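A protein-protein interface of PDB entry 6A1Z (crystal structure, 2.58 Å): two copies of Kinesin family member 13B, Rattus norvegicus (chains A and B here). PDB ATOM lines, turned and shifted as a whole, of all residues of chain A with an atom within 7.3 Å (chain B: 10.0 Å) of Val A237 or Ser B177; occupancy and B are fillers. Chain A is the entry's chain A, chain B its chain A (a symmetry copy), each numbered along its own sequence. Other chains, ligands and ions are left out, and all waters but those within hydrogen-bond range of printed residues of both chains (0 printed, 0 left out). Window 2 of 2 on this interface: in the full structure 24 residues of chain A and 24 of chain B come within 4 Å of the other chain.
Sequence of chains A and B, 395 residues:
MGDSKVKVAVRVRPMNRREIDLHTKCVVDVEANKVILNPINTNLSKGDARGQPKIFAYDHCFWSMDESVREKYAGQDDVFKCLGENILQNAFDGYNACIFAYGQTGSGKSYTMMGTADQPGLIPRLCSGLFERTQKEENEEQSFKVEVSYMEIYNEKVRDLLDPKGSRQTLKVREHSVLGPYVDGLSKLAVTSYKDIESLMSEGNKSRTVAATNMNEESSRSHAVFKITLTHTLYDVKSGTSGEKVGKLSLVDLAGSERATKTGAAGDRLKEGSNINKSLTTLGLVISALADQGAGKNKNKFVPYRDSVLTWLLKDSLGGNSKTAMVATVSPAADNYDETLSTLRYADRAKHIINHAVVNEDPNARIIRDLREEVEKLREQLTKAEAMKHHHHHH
NE2 of His B176 sits at hydrogen-bond distance from O of Glu A140, 2.9 Å away.
ND1 of His B176 lies close to N of Leu B179 (3.3 Å).
The backbone NH (N) of Tyr A235 sits at hydrogen-bond distance from the backbone carbonyl oxygen (O) of Glu A141 (3.1 Å).
The backbone NH (N) of Ser A239 sits at hydrogen-bond distance from the side-chain carboxylate (OD2) of Asp A236, at 3.4 Å.
O of Thr A241 sits at hydrogen-bond distance from N of Asp A236 (3.0 Å).
CG1 of Val B178 touches CD1 of Tyr A235, at 3.7 Å.
Leu B179 touches Tyr A235.
Val B178 touches Asp A236.
Val A237 touches Ser B177 (O to CB, 3.6 Å).
Ser B177 touches Gly A240 (O to CA, 3.7 Å).
Val B178 touches Gly A240.
CG2 of Val B178 touches O of Thr A241, at 3.6 Å.
Of chain B, only Ser B177 (3.6 Å) comes within 4 Å of Val A237.
Of chain A, only Val A237 (3.6 Å) and Gly A240 (3.7 Å) come within 4 Å of Ser B177.
Asp A236 touches just one residue of chain B: Val B178 (3.98 Å).
Lys A238 touches none of the printed residues of chain B.
Ser A239 touches none of the printed residues of chain B.
Printed residues of chain B within 4 Å of Gly A240: Ser B177 and Val B178.
Printed residues of chain B within 4 Å of Glu A140: His B176 (2.9 Å).
Of the printed residues of chain A, His B176 touches Glu A140 (2.9 Å).
Gly B180 touches none of the printed residues of chain A.
The nearest printed residue of chain B that does not touch Thr A241 is Ser B177 (5.4 Å).
Of the 9 printed residues of chain B, 4 touch a printed residue of chain A.
Hydrophobic or aromatic side chains of chain B that line the printed part of chain A: His B176, Val B178 and Leu B179.
Printed residues of chain A that touch a printed residue of chain B: Glu A140, Tyr A235, Asp A236, Val A237, Gly A240 and Thr A241.
Hydrophobic or aromatic side chains of chain A within 4 Å of the printed part of chain B: Tyr A235 and Val A237.
Among the printed residues, 8 pairs touch across the chains.
Among the printed residues, no Asp or Glu carboxylate lies within 4 Å of a Lys or Arg side-chain nitrogen of the other chain.
No position is printed for both chains.
Of the 8 pairs that touch across the chains among the printed residues, none has its exchanged pair printed and touching as well.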
ATOM      1  N   GLU A 140       3.901   4.873  12.924  1.00  0.00           N
ATOM      2  CA  GLU A 140       2.583   5.149  13.500  1.00  0.00           C
ATOM      3  C   GLU A 140       1.606   5.657  12.443  1.00  0.00           C
ATOM      4  O   GLU A 140       0.427   5.877  12.737  1.00  0.00           O
ATOM      5  CB  GLU A 140       2.675   6.145  14.670  1.00  0.00           C
ATOM      6  N   GLU A 141       2.086   5.847  11.214  1.00  0.00           N
ATOM      7  CA  GLU A 141       1.225   5.976  10.047  1.00  0.00           C
ATOM      8  C   GLU A 141       1.327   4.781   9.096  1.00  0.00           C
ATOM      9  O   GLU A 141       0.477   4.655   8.204  1.00  0.00           O
ATOM     10  CB  GLU A 141       1.547   7.275   9.279  1.00  0.00           C
ATOM     11  CG  GLU A 141       1.475   8.550  10.111  1.00  0.00           C
ATOM     12  CD  GLU A 141       2.148   9.752   9.440  1.00  0.00           C
ATOM     13  OE1 GLU A 141       1.693  10.182   8.352  1.00  0.00           O
ATOM     14  OE2 GLU A 141       3.134  10.269  10.016  1.00  0.00           O
ATOM     15  N   LEU A 234      -1.637   1.614   5.791  1.00  0.00           N
ATOM     16  CA  LEU A 234      -1.555   3.068   5.822  1.00  0.00           C
ATOM     17  C   LEU A 234      -2.734   3.609   6.612  1.00  0.00           C
ATOM     18  O   LEU A 234      -3.855   3.108   6.497  1.00  0.00           O
ATOM     19  CB  LEU A 234      -1.537   3.654   4.403  1.00  0.00           C
ATOM     20  CG  LEU A 234      -0.303   3.280   3.572  1.00  0.00           C
ATOM     21  CD1 LEU A 234      -0.567   2.045   2.731  1.00  0.00           C
ATOM     22  CD2 LEU A 234       0.175   4.436   2.711  1.00  0.00           C
ATOM     23  N   TYR A 235      -2.475   4.613   7.435  1.00  0.00           N
ATOM     24  CA  TYR A 235      -3.485   5.153   8.333  1.00  0.00           C
ATOM     25  C   TYR A 235      -3.770   6.608   7.980  1.00  0.00           C
ATOM     26  O   TYR A 235      -2.848   7.426   7.882  1.00  0.00           O
ATOM     27  CB  TYR A 235      -3.040   5.009   9.792  1.00  0.00           C
ATOM     28  CG  TYR A 235      -2.748   3.569  10.185  1.00  0.00           C
ATOM     29  CD1 TYR A 235      -3.714   2.787  10.823  1.00  0.00           C
ATOM     30  CD2 TYR A 235      -1.510   2.983   9.900  1.00  0.00           C
ATOM     31  CE1 TYR A 235      -3.452   1.462  11.184  1.00  0.00           C
ATOM     32  CE2 TYR A 235      -1.230   1.653  10.248  1.00  0.00           C
ATOM     33  CZ  TYR A 235      -2.205   0.899  10.892  1.00  0.00           C
ATOM     34  OH  TYR A 235      -1.930  -0.410  11.244  1.00  0.00           O
ATOM     35  N   ASP A 236      -5.048   6.905   7.745  1.00  0.00           N
ATOM     36  CA  ASP A 236      -5.564   8.269   7.601  1.00  0.00           C
ATOM     37  C   ASP A 236      -5.930   8.722   9.008  1.00  0.00           C
ATOM     38  O   ASP A 236      -7.059   8.535   9.452  1.00  0.00           O
ATOM     39  CB  ASP A 236      -6.778   8.300   6.667  1.00  0.00           C
ATOM     40  CG  ASP A 236      -6.989   9.653   5.975  1.00  0.00           C
ATOM     41  OD1 ASP A 236      -7.699   9.667   4.935  1.00  0.00           O
ATOM     42  OD2 ASP A 236      -6.472  10.688   6.458  1.00  0.00           O
ATOM     43  N   VAL A 237      -4.961   9.309   9.723  1.00  0.00           N
ATOM     44  CA  VAL A 237      -5.208   9.714  11.113  1.00  0.00           C
ATOM     45  C   VAL A 237      -6.232  10.852  11.177  1.00  0.00           C
ATOM     46  O   VAL A 237      -6.924  11.023  12.193  1.00  0.00           O
ATOM     47  CB  VAL A 237      -3.885  10.099  11.822  1.00  0.00           C
ATOM     48  CG1 VAL A 237      -4.120  10.464  13.298  1.00  0.00           C
ATOM     49  CG2 VAL A 237      -2.854   8.984  11.703  1.00  0.00           C
ATOM     50  N   LYS A 238      -6.338  11.651  10.106  1.00  0.00           N
ATOM     51  CA  LYS A 238      -7.385  12.664  10.031  1.00  0.00           C
ATOM     52  C   LYS A 238      -8.745  12.019   9.799  1.00  0.00           C
ATOM     53  O   LYS A 238      -9.714  12.318  10.507  1.00  0.00           O
ATOM     54  CB  LYS A 238      -7.067  13.676   8.925  1.00  0.00           C
ATOM     55  N   SER A 239      -8.839  11.118   8.819  1.00  0.00           N
ATOM     56  CA  SER A 239     -10.111  10.454   8.562  1.00  0.00           C
ATOM     57  C   SER A 239     -10.377   9.278   9.503  1.00  0.00           C
ATOM     58  O   SER A 239     -11.518   8.816   9.573  1.00  0.00           O
ATOM     59  CB  SER A 239     -10.184   9.988   7.105  1.00  0.00           C
ATOM     60  N   GLY A 240      -9.367   8.796  10.232  1.00  0.00           N
ATOM     61  CA  GLY A 240      -9.551   7.675  11.142  1.00  0.00           C
ATOM     62  C   GLY A 240      -9.720   6.320  10.486  1.00  0.00           C
ATOM     63  O   GLY A 240     -10.140   5.370  11.151  1.00  0.00           O
ATOM     64  N   THR A 241      -9.392   6.194   9.202  1.00  0.00           N
ATOM     65  CA  THR A 241      -9.598   4.975   8.432  1.00  0.00           C
ATOM     66  C   THR A 241      -8.258   4.303   8.105  1.00  0.00           C
ATOM     67  O   THR A 241      -7.175   4.829   8.387  1.00  0.00           O
ATOM     68  CB  THR A 241     -10.393   5.296   7.163  1.00  0.00           C
ATOM     69  N   ARG B 174       0.197   4.697  23.988  1.00  0.00           N
ATOM     70  CA  ARG B 174      -0.178   5.827  23.152  1.00  0.00           C
ATOM     71  C   ARG B 174      -1.650   5.728  22.779  1.00  0.00           C
ATOM     72  O   ARG B 174      -2.303   4.699  22.971  1.00  0.00           O
ATOM     73  CB  ARG B 174       0.686   5.910  21.882  1.00  0.00           C
ATOM     74  CG  ARG B 174       2.174   5.551  22.061  1.00  0.00           C
ATOM     75  CD  ARG B 174       2.874   6.447  23.077  1.00  0.00           C
ATOM     76  NE  ARG B 174       4.165   6.980  22.629  1.00  0.00           N
ATOM     77  CZ  ARG B 174       4.871   7.881  23.319  1.00  0.00           C
ATOM     78  NH1 ARG B 174       4.404   8.343  24.480  1.00  0.00           N
ATOM     79  NH2 ARG B 174       6.041   8.318  22.855  1.00  0.00           N
ATOM     80  N   GLU B 175      -2.177   6.831  22.270  1.00  0.00           N
ATOM     81  CA  GLU B 175      -3.516   6.867  21.712  1.00  0.00           C
ATOM     82  C   GLU B 175      -3.400   6.919  20.195  1.00  0.00           C
ATOM     83  O   GLU B 175      -2.344   7.235  19.642  1.00  0.00           O
ATOM     84  CB  GLU B 175      -4.308   8.058  22.265  1.00  0.00           C
ATOM     85  N   HIS B 176      -4.490   6.577  19.517  1.00  0.00           N
ATOM     86  CA  HIS B 176      -4.481   6.504  18.060  1.00  0.00           C
ATOM     87  C   HIS B 176      -5.906   6.682  17.557  1.00  0.00           C
ATOM     88  O   HIS B 176      -6.858   6.195  18.182  1.00  0.00           O
ATOM     89  CB  HIS B 176      -3.908   5.166  17.568  1.00  0.00           C
ATOM     90  CG  HIS B 176      -3.149   5.250  16.279  1.00  0.00           C
ATOM     91  ND1 HIS B 176      -3.425   4.426  15.211  1.00  0.00           N
ATOM     92  CD2 HIS B 176      -2.086   6.003  15.908  1.00  0.00           C
ATOM     93  CE1 HIS B 176      -2.592   4.695  14.221  1.00  0.00           C
ATOM     94  NE2 HIS B 176      -1.766   5.645  14.621  1.00  0.00           N
ATOM     95  N   SER B 177      -6.041   7.363  16.417  1.00  0.00           N
ATOM     96  CA  SER B 177      -7.355   7.609  15.843  1.00  0.00           C
ATOM     97  C   SER B 177      -7.863   6.446  14.992  1.00  0.00           C
ATOM     98  O   SER B 177      -9.029   6.473  14.573  1.00  0.00           O
ATOM     99  CB  SER B 177      -7.313   8.909  15.033  1.00  0.00           C
ATOM    100  OG  SER B 177      -6.731   9.971  15.797  1.00  0.00           O
ATOM    101  N   VAL B 178      -7.033   5.423  14.743  1.00  0.00           N
ATOM    102  CA  VAL B 178      -7.451   4.245  13.980  1.00  0.00           C
ATOM    103  C   VAL B 178      -7.327   2.981  14.830  1.00  0.00           C
ATOM    104  O   VAL B 178      -8.144   2.058  14.703  1.00  0.00           O
ATOM    105  CB  VAL B 178      -6.658   4.100  12.659  1.00  0.00           C
ATOM    106  CG1 VAL B 178      -7.265   2.996  11.775  1.00  0.00           C
ATOM    107  CG2 VAL B 178      -6.586   5.431  11.896  1.00  0.00           C
ATOM    108  N   LEU B 179      -6.308   2.921  15.699  1.00  0.00           N
ATOM    109  CA  LEU B 179      -6.121   1.785  16.606  1.00  0.00           C
ATOM    110  C   LEU B 179      -6.707   2.009  18.007  1.00  0.00           C
ATOM    111  O   LEU B 179      -7.028   1.027  18.692  1.00  0.00           O
ATOM    112  CB  LEU B 179      -4.621   1.434  16.744  1.00  0.00           C
ATOM    113  CG  LEU B 179      -3.620   1.306  15.569  1.00  0.00           C
ATOM    114  CD1 LEU B 179      -2.184   1.149  16.097  1.00  0.00           C
ATOM    115  CD2 LEU B 179      -3.955   0.179  14.573  1.00  0.00           C
ATOM    116  N   GLY B 180      -6.877   3.263  18.437  1.00  0.00           N
ATOM    117  CA  GLY B 180      -7.207   3.557  19.808  1.00  0.00           C
ATOM    118  C   GLY B 180      -5.956   3.527  20.657  1.00  0.00           C
ATOM    119  O   GLY B 180      -4.832   3.590  20.146  1.00  0.00           O
ATOM    120  N   PRO B 181      -6.116   3.412  21.974  1.00  0.00           N
ATOM    121  CA  PRO B 181      -4.936   3.319  22.845  1.00  0.00           C
ATOM    122  C   PRO B 181      -4.200   2.009  22.593  1.00  0.00           C
ATOM    123  O   PRO B 181      -4.813   0.937  22.539  1.00  0.00           O
ATOM    124  CB  PRO B 181      -5.527   3.380  24.254  1.00  0.00           C
ATOM    125  CG  PRO B 181      -6.910   2.793  24.098  1.00  0.00           C
ATOM    126  CD  PRO B 181      -7.373   3.130  22.697  1.00  0.00           C
ATOM    127  N   TYR B 182      -2.882   2.104  22.412  1.00  0.00           N
ATOM    128  CA  TYR B 182      -2.066   0.931  22.128  1.00  0.00           C
ATOM    129  C   TYR B 182      -0.739   1.022  22.869  1.00  0.00           C
ATOM    130  O   TYR B 182      -0.267   2.107  23.220  1.00  0.00           O
ATOM    131  CB  TYR B 182      -1.805   0.762  20.623  1.00  0.00           C
ATOM    132  CG  TYR B 182      -0.901   1.817  20.044  1.00  0.00           C
ATOM    133  CD1 TYR B 182      -1.392   3.073  19.731  1.00  0.00           C
ATOM    134  CD2 TYR B 182       0.444   1.565  19.820  1.00  0.00           C
ATOM    135  CE1 TYR B 182      -0.568   4.051  19.202  1.00  0.00           C
ATOM    136  CE2 TYR B 182       1.278   2.536  19.290  1.00  0.00           C
ATOM    137  CZ  TYR B 182       0.766   3.780  18.980  1.00  0.00           C
ATOM    138  OH  TYR B 182       1.580   4.762  18.455  1.00  0.00           O
